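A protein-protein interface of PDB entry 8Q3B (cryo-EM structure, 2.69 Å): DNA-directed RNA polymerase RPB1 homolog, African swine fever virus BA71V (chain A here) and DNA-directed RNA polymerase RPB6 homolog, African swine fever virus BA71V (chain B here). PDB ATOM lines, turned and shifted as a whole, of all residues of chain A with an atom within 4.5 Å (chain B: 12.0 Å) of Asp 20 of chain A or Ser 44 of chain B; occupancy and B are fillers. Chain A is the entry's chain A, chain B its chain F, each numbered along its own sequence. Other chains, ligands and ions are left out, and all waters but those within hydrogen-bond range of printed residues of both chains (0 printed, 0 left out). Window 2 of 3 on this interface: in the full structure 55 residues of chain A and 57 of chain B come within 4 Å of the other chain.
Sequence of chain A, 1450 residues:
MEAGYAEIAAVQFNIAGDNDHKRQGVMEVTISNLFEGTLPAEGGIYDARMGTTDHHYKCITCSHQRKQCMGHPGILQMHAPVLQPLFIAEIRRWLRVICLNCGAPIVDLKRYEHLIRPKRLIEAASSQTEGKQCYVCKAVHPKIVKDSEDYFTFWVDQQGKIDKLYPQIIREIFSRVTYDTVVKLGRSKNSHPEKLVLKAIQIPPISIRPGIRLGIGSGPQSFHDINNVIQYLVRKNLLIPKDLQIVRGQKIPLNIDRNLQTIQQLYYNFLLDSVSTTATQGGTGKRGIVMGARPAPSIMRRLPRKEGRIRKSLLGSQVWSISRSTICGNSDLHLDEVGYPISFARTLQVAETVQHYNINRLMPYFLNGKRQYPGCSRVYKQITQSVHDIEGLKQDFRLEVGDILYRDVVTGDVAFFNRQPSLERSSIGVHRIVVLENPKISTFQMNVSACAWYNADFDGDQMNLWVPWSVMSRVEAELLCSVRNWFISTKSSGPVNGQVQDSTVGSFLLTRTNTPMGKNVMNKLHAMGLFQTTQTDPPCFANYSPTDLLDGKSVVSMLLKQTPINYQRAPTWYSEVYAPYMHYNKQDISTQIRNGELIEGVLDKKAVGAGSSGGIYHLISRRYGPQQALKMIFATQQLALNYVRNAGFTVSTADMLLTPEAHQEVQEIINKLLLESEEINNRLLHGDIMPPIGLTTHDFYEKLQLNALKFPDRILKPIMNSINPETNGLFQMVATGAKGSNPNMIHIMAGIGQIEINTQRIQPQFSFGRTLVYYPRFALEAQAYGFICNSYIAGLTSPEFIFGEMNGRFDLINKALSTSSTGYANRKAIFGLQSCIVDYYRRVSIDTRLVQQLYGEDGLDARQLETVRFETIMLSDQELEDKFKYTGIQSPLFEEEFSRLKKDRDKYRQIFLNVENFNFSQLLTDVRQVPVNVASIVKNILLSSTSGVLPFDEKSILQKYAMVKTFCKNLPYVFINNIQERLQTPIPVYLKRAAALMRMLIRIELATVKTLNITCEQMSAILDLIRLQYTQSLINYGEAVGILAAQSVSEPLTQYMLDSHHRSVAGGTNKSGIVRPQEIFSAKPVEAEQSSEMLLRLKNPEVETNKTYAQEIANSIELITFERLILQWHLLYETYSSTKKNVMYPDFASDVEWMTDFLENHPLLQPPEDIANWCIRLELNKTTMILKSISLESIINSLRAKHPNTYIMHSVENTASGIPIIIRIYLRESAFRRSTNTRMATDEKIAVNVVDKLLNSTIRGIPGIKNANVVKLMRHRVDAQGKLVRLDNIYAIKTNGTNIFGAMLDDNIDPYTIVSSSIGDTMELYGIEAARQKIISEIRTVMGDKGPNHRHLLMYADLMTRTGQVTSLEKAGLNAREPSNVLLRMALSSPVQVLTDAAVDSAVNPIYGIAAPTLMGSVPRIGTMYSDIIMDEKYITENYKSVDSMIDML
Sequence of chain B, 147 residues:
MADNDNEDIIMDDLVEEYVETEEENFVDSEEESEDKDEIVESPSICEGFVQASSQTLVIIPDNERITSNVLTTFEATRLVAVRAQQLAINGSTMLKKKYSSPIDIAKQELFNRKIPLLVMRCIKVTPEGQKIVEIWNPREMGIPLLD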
ATOM      1  N   ILE A  15       6.537   5.913  17.367  1.00  0.00           N
ATOM      2  CA  ILE A  15       5.819   5.258  18.453  1.00  0.00           C
ATOM      3  C   ILE A  15       6.582   4.002  18.846  1.00  0.00           C
ATOM      4  O   ILE A  15       6.866   3.143  18.001  1.00  0.00           O
ATOM      5  CB  ILE A  15       4.377   4.928  18.035  1.00  0.00           C
ATOM      6  CG1 ILE A  15       3.604   6.212  17.730  1.00  0.00           C
ATOM      7  CG2 ILE A  15       3.670   4.145  19.132  1.00  0.00           C
ATOM      8  CD1 ILE A  15       2.303   5.984  16.991  1.00  0.00           C
ATOM      9  N   ALA A  16       6.918   3.890  20.127  1.00  0.00           N
ATOM     10  CA  ALA A  16       7.709   2.775  20.627  1.00  0.00           C
ATOM     11  C   ALA A  16       6.780   1.649  21.062  1.00  0.00           C
ATOM     12  O   ALA A  16       6.004   1.809  22.010  1.00  0.00           O
ATOM     13  CB  ALA A  16       8.594   3.221  21.789  1.00  0.00           C
ATOM     14  N   GLY A  17       6.860   0.515  20.371  1.00  0.00           N
ATOM     15  CA  GLY A  17       6.087  -0.650  20.734  1.00  0.00           C
ATOM     16  C   GLY A  17       6.751  -1.449  21.836  1.00  0.00           C
ATOM     17  O   GLY A  17       7.822  -1.114  22.339  1.00  0.00           O
ATOM     18  N   ASP A  18       6.086  -2.541  22.218  1.00  0.00           N
ATOM     19  CA  ASP A  18       6.639  -3.397  23.264  1.00  0.00           C
ATOM     20  C   ASP A  18       7.912  -4.093  22.801  1.00  0.00           C
ATOM     21  O   ASP A  18       8.766  -4.427  23.628  1.00  0.00           O
ATOM     22  CB  ASP A  18       5.608  -4.432  23.717  1.00  0.00           C
ATOM     23  CG  ASP A  18       4.824  -5.024  22.564  1.00  0.00           C
ATOM     24  OD1 ASP A  18       4.869  -4.449  21.456  1.00  0.00           O
ATOM     25  OD2 ASP A  18       4.161  -6.063  22.767  1.00  0.00           O
ATOM     26  N   ASN A  19       8.057  -4.321  21.494  1.00  0.00           N
ATOM     27  CA  ASN A  19       9.285  -4.924  20.988  1.00  0.00           C
ATOM     28  C   ASN A  19      10.484  -4.026  21.258  1.00  0.00           C
ATOM     29  O   ASN A  19      11.552  -4.504  21.662  1.00  0.00           O
ATOM     30  CB  ASN A  19       9.154  -5.203  19.490  1.00  0.00           C
ATOM     31  CG  ASN A  19       8.654  -6.604  19.197  1.00  0.00           C
ATOM     32  OD1 ASN A  19       8.568  -7.448  20.088  1.00  0.00           O
ATOM     33  ND2 ASN A  19       8.319  -6.858  17.938  1.00  0.00           N
ATOM     34  N   ASP A  20      10.329  -2.718  21.040  1.00  0.00           N
ATOM     35  CA  ASP A  20      11.408  -1.787  21.340  1.00  0.00           C
ATOM     36  C   ASP A  20      11.758  -1.814  22.821  1.00  0.00           C
ATOM     37  O   ASP A  20      12.938  -1.800  23.189  1.00  0.00           O
ATOM     38  CB  ASP A  20      11.015  -0.373  20.912  1.00  0.00           C
ATOM     39  CG  ASP A  20      10.715  -0.275  19.429  1.00  0.00           C
ATOM     40  OD1 ASP A  20      11.653  -0.427  18.620  1.00  0.00           O
ATOM     41  OD2 ASP A  20       9.540  -0.046  19.073  1.00  0.00           O
ATOM     42  N   HIS A  21      10.744  -1.852  23.687  1.00  0.00           N
ATOM     43  CA  HIS A  21      11.000  -1.899  25.121  1.00  0.00           C
ATOM     44  C   HIS A  21      11.752  -3.167  25.504  1.00  0.00           C
ATOM     45  O   HIS A  21      12.705  -3.120  26.289  1.00  0.00           O
ATOM     46  CB  HIS A  21       9.681  -1.810  25.887  1.00  0.00           C
ATOM     47  CG  HIS A  21       8.969  -0.505  25.711  1.00  0.00           C
ATOM     48  ND1 HIS A  21       9.551   0.584  25.100  1.00  0.00           N
ATOM     49  CD2 HIS A  21       7.721  -0.117  26.062  1.00  0.00           C
ATOM     50  CE1 HIS A  21       8.693   1.588  25.085  1.00  0.00           C
ATOM     51  NE2 HIS A  21       7.574   1.188  25.663  1.00  0.00           N
ATOM     52  N   LYS A  22      11.338  -4.312  24.957  1.00  0.00           N
ATOM     53  CA  LYS A  22      12.010  -5.567  25.275  1.00  0.00           C
ATOM     54  C   LYS A  22      13.450  -5.561  24.784  1.00  0.00           C
ATOM     55  O   LYS A  22      14.355  -6.035  25.483  1.00  0.00           O
ATOM     56  CB  LYS A  22      11.244  -6.741  24.667  1.00  0.00           C
ATOM     57  CG  LYS A  22       9.884  -6.985  25.295  1.00  0.00           C
ATOM     58  CD  LYS A  22       9.276  -8.300  24.819  1.00  0.00           C
ATOM     59  CE  LYS A  22       8.043  -8.095  23.943  1.00  0.00           C
ATOM     60  NZ  LYS A  22       6.818  -8.666  24.565  1.00  0.00           N
ATOM     61  N   ARG A  23      13.686  -5.034  23.582  1.00  0.00           N
ATOM     62  CA  ARG A  23      15.033  -5.051  23.023  1.00  0.00           C
ATOM     63  C   ARG A  23      15.958  -4.087  23.758  1.00  0.00           C
ATOM     64  O   ARG A  23      17.110  -4.429  24.053  1.00  0.00           O
ATOM     65  CB  ARG A  23      14.977  -4.711  21.534  1.00  0.00           C
ATOM     66  CG  ARG A  23      16.116  -5.296  20.723  1.00  0.00           C
ATOM     67  CD  ARG A  23      16.227  -4.633  19.361  1.00  0.00           C
ATOM     68  NE  ARG A  23      15.832  -5.533  18.285  1.00  0.00           N
ATOM     69  CZ  ARG A  23      16.596  -6.504  17.804  1.00  0.00           C
ATOM     70  NH1 ARG A  23      17.804  -6.740  18.290  1.00  0.00           N
ATOM     71  NH2 ARG A  23      16.136  -7.258  16.810  1.00  0.00           N
ATOM     72  N   GLN A  24      15.475  -2.882  24.064  1.00  0.00           N
ATOM     73  CA  GLN A  24      16.336  -1.871  24.669  1.00  0.00           C
ATOM     74  C   GLN A  24      16.586  -2.140  26.147  1.00  0.00           C
ATOM     75  O   GLN A  24      17.683  -1.866  26.646  1.00  0.00           O
ATOM     76  CB  GLN A  24      15.716  -0.487  24.490  1.00  0.00           C
ATOM     77  CG  GLN A  24      15.766   0.028  23.065  1.00  0.00           C
ATOM     78  CD  GLN A  24      14.894   1.248  22.861  1.00  0.00           C
ATOM     79  OE1 GLN A  24      14.992   2.226  23.601  1.00  0.00           O
ATOM     80  NE2 GLN A  24      14.035   1.197  21.852  1.00  0.00           N
ATOM     81  N   LYS A 195       0.846  -1.637  17.655  1.00  0.00           N
ATOM     82  CA  LYS A 195       1.752  -1.254  18.736  1.00  0.00           C
ATOM     83  C   LYS A 195       1.172  -0.189  19.648  1.00  0.00           C
ATOM     84  O   LYS A 195       1.913   0.318  20.498  1.00  0.00           O
ATOM     85  CB  LYS A 195       3.087  -0.772  18.164  1.00  0.00           C
ATOM     86  CG  LYS A 195       2.991   0.459  17.280  1.00  0.00           C
ATOM     87  CD  LYS A 195       4.349   1.109  17.075  1.00  0.00           C
ATOM     88  CE  LYS A 195       5.260   0.253  16.212  1.00  0.00           C
ATOM     89  NZ  LYS A 195       6.663   0.748  16.223  1.00  0.00           N
ATOM     90  N   VAL B  40      -0.299  -8.999  12.580  1.00  0.00           N
ATOM     91  CA  VAL B  40       0.857  -8.126  12.418  1.00  0.00           C
ATOM     92  C   VAL B  40       1.491  -7.906  13.783  1.00  0.00           C
ATOM     93  O   VAL B  40       0.810  -7.497  14.731  1.00  0.00           O
ATOM     94  CB  VAL B  40       0.465  -6.781  11.778  1.00  0.00           C
ATOM     95  CG1 VAL B  40       1.648  -5.822  11.779  1.00  0.00           C
ATOM     96  CG2 VAL B  40      -0.055  -6.997  10.366  1.00  0.00           C
ATOM     97  N   GLU B  41       2.789  -8.177  13.878  1.00  0.00           N
ATOM     98  CA  GLU B  41       3.591  -7.841  15.048  1.00  0.00           C
ATOM     99  C   GLU B  41       4.585  -6.767  14.632  1.00  0.00           C
ATOM    100  O   GLU B  41       5.398  -6.986  13.727  1.00  0.00           O
ATOM    101  CB  GLU B  41       4.312  -9.071  15.598  1.00  0.00           C
ATOM    102  CG  GLU B  41       5.129  -8.804  16.853  1.00  0.00           C
ATOM    103  CD  GLU B  41       5.944 -10.007  17.285  1.00  0.00           C
ATOM    104  OE1 GLU B  41       6.805 -10.457  16.500  1.00  0.00           O
ATOM    105  OE2 GLU B  41       5.725 -10.503  18.411  1.00  0.00           O
ATOM    106  N   SER B  42       4.524  -5.619  15.289  1.00  0.00           N
ATOM    107  CA  SER B  42       5.320  -4.473  14.867  1.00  0.00           C
ATOM    108  C   SER B  42       6.799  -4.730  15.126  1.00  0.00           C
ATOM    109  O   SER B  42       7.176  -4.999  16.275  1.00  0.00           O
ATOM    110  CB  SER B  42       4.861  -3.220  15.602  1.00  0.00           C
ATOM    111  OG  SER B  42       3.448  -3.117  15.589  1.00  0.00           O
ATOM    112  N   PRO B  43       7.664  -4.664  14.116  1.00  0.00           N
ATOM    113  CA  PRO B  43       9.099  -4.829  14.368  1.00  0.00           C
ATOM    114  C   PRO B  43       9.678  -3.633  15.107  1.00  0.00           C
ATOM    115  O   PRO B  43       9.089  -2.550  15.165  1.00  0.00           O
ATOM    116  CB  PRO B  43       9.703  -4.953  12.963  1.00  0.00           C
ATOM    117  CG  PRO B  43       8.552  -5.226  12.055  1.00  0.00           C
ATOM    118  CD  PRO B  43       7.381  -4.548  12.676  1.00  0.00           C
ATOM    119  N   SER B  44      10.858  -3.848  15.681  1.00  0.00           N
ATOM    120  CA  SER B  44      11.569  -2.763  16.340  1.00  0.00           C
ATOM    121  C   SER B  44      11.949  -1.691  15.325  1.00  0.00           C
ATOM    122  O   SER B  44      12.178  -1.971  14.145  1.00  0.00           O
ATOM    123  CB  SER B  44      12.820  -3.297  17.039  1.00  0.00           C
ATOM    124  OG  SER B  44      13.535  -2.250  17.672  1.00  0.00           O
ATOM    125  N   ILE B  45      12.014  -0.445  15.797  1.00  0.00           N
ATOM    126  CA  ILE B  45      12.329   0.667  14.904  1.00  0.00           C
ATOM    127  C   ILE B  45      13.734   0.514  14.340  1.00  0.00           C
ATOM    128  O   ILE B  45      13.994   0.849  13.177  1.00  0.00           O
ATOM    129  CB  ILE B  45      12.160   2.020  15.624  1.00  0.00           C
ATOM    130  CG1 ILE B  45      10.863   2.074  16.447  1.00  0.00           C
ATOM    131  CG2 ILE B  45      12.214   3.161  14.617  1.00  0.00           C
ATOM    132  CD1 ILE B  45       9.614   2.299  15.621  1.00  0.00           C
ATOM    133  N   CYS B  46      14.666   0.011  15.154  1.00  0.00           N
ATOM    134  CA  CYS B  46      16.054  -0.110  14.715  1.00  0.00           C
ATOM    135  C   CYS B  46      16.166  -0.922  13.432  1.00  0.00           C
ATOM    136  O   CYS B  46      17.004  -0.628  12.573  1.00  0.00           O
ATOM    137  CB  CYS B  46      16.889  -0.750  15.820  1.00  0.00           C
ATOM    138  SG  CYS B  46      16.229  -2.329  16.401  1.00  0.00           S
ATOM    139  N   GLU B  47      15.330  -1.951  13.280  1.00  0.00           N
ATOM    140  CA  GLU B  47      15.421  -2.805  12.099  1.00  0.00           C
ATOM    141  C   GLU B  47      15.146  -2.016  10.828  1.00  0.00           C
ATOM    142  O   GLU B  47      15.828  -2.204   9.812  1.00  0.00           O
ATOM    143  CB  GLU B  47      14.445  -3.976  12.221  1.00  0.00           C
ATOM    144  CG  GLU B  47      14.558  -4.839  13.491  1.00  0.00           C
ATOM    145  CD  GLU B  47      15.963  -4.961  14.079  1.00  0.00           C
ATOM    146  OE1 GLU B  47      16.963  -4.645  13.401  1.00  0.00           O
ATOM    147  OE2 GLU B  47      16.061  -5.379  15.249  1.00  0.00           O
ATOM    148  N   GLY B  48      14.154  -1.130  10.860  1.00  0.00           N
ATOM    149  CA  GLY B  48      13.841  -0.315   9.702  1.00  0.00           C
ATOM    150  C   GLY B  48      14.762   0.863   9.483  1.00  0.00           C
ATOM    151  O   GLY B  48      14.656   1.531   8.451  1.00  0.00           O
ATOM    152  N   PHE B  49      15.659   1.132  10.427  1.00  0.00           N
ATOM    153  CA  PHE B  49      16.574   2.260  10.316  1.00  0.00           C
ATOM    154  C   PHE B  49      17.789   1.879   9.482  1.00  0.00           C
ATOM    155  O   PHE B  49      18.413   0.839   9.715  1.00  0.00           O
ATOM    156  CB  PHE B  49      17.015   2.719  11.704  1.00  0.00           C
ATOM    157  CG  PHE B  49      18.007   3.843  11.685  1.00  0.00           C
ATOM    158  CD1 PHE B  49      17.604   5.134  11.396  1.00  0.00           C
ATOM    159  CD2 PHE B  49      19.344   3.608  11.951  1.00  0.00           C
ATOM    160  CE1 PHE B  49      18.517   6.168  11.378  1.00  0.00           C
ATOM    161  CE2 PHE B  49      20.258   4.639  11.934  1.00  0.00           C
ATOM    162  CZ  PHE B  49      19.844   5.920  11.647  1.00  0.00           C
ATOM    163  N   VAL B  50      18.125   2.726   8.511  1.00  0.00           N
ATOM    164  CA  VAL B  50      19.329   2.578   7.703  1.00  0.00           C
ATOM    165  C   VAL B  50      20.175   3.830   7.887  1.00  0.00           C
ATOM    166  O   VAL B  50      19.684   4.950   7.711  1.00  0.00           O
ATOM    167  CB  VAL B  50      18.997   2.342   6.217  1.00  0.00           C
ATOM    168  CG1 VAL B  50      17.892   1.308   6.076  1.00  0.00           C
ATOM    169  CG2 VAL B  50      18.589   3.642   5.536  1.00  0.00           C
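Hydrophobic or aromatic side chains of chain B that line the printed part of chain A: Ile 45.
Among the printed residues, 10 pairs touch across the chains.
Among the printed residues, Asp or Glu carboxylates within 4 Å of a Lys or Arg side-chain nitrogen of the other chain: Arg 23 of chain A with Glu 47 of chain B (2.4 Å).
Among the printed residues, merely in contact across the chains: Ile 15 of chain A with Ile 45 of chain B (3.7 Å), Asn 19 of chain A with Glu 41 of chain B (3.9 Å), Arg 23 of chain A with Ser 44 of chain B (3.95 Å), Lys 195 of chain A with Ser 42 of chain B (3.5 Å) and Lys 195 of chain A with Ile 45 of chain B (3.4 Å).
O of Ser 42 of chain B is in hydrogen-bond range of ND2 of Asn 19 of chain A, 2.7 Å away.
The side-chain carboxylate (OD1) of Asp 20 of chain A is in hydrogen-bond range of the side-chain hydroxyl (OG) of Ser 44 of chain B.
The side-chain carboxylate (OD1) of Asp 20 of chain A sits at hydrogen-bond distance from the backbone NH (N) of Ile 45 of chain B (2.8 Å).
The guanidinium group (NE) of Arg 23 of chain A lies within hydrogen-bond range of the side-chain sulfur (SG) of Cys 46 of chain B, 3.7 Å away.
NH2 of Arg 23 of chain A is in salt-bridge range of OE2 of Glu 47 of chain B, at 2.4 Å.
Of the printed residues of chain B, Ile 15 of chain A touches Ile 45.
Ala 16 of chain A touches none of the printed residues of chain B.
No residue of chain B comes within 4 Å of Asp 18 of chain A.
Of chain B, only Glu 41 (3.9 Å) and Ser 42 (2.7 Å) come within 4 Å of Asn 19 of chain A.
Asp 20 of chain A touches two residues of chain B.
No residue of chain B comes within 4 Å of His 21 of chain A.
No residue of chain B comes within 4 Å of Lys 22 of chain A.
Arg 23 of chain A touches just these residues of chain B: Ser 44 (3.95 Å), Cys 46 (3.7 Å) and Glu 47 (2.4 Å).
No residue of chain B comes within 4 Å of Gln 24 of chain A.
Of the printed residues of chain B, Lys 195 of chain A touches Ser 42 and Ile 45.
Printed residues of chain A within 4 Å of Glu 41 of chain B: Asn 19 (3.9 Å).
Ser 44 of chain B touches just these residues of chain A: Asp 20 (2.8 Å) and Arg 23 (3.95 Å).
Printed residues of chain A within 4 Å of Glu 47 of chain B: Arg 23.
Val 50 of chain B touches none of the printed residues of chain A.
The nearest residue of chain B that does not touch Asp 20 of chain A is Cys 46 of chain B (4.6 Å).
The side-chain amino group (NZ) of Lys 195 of chain A is in hydrogen-bond range of the backbone carbonyl oxygen (O) of Ile 15 of chain A (3.0 Å).
The side-chain carboxylate of Asp 20 of chain A is in hydrogen-bond range of the backbone NH of Gly 17 of chain A, at 3.0 Å.
O of Asp 20 of chain A lies close to NE2 of Gln 24 of chain A (3.5 Å).
The side-chain hydroxyl of Ser 44 of chain B lies within hydrogen-bond range of the side-chain sulfur of Cys 46 of chain B, 3.0 Å away.
SG of Cys 46 of chain B is in hydrogen-bond range of OE2 of Glu 47 of chain B, at 3.3 Å.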
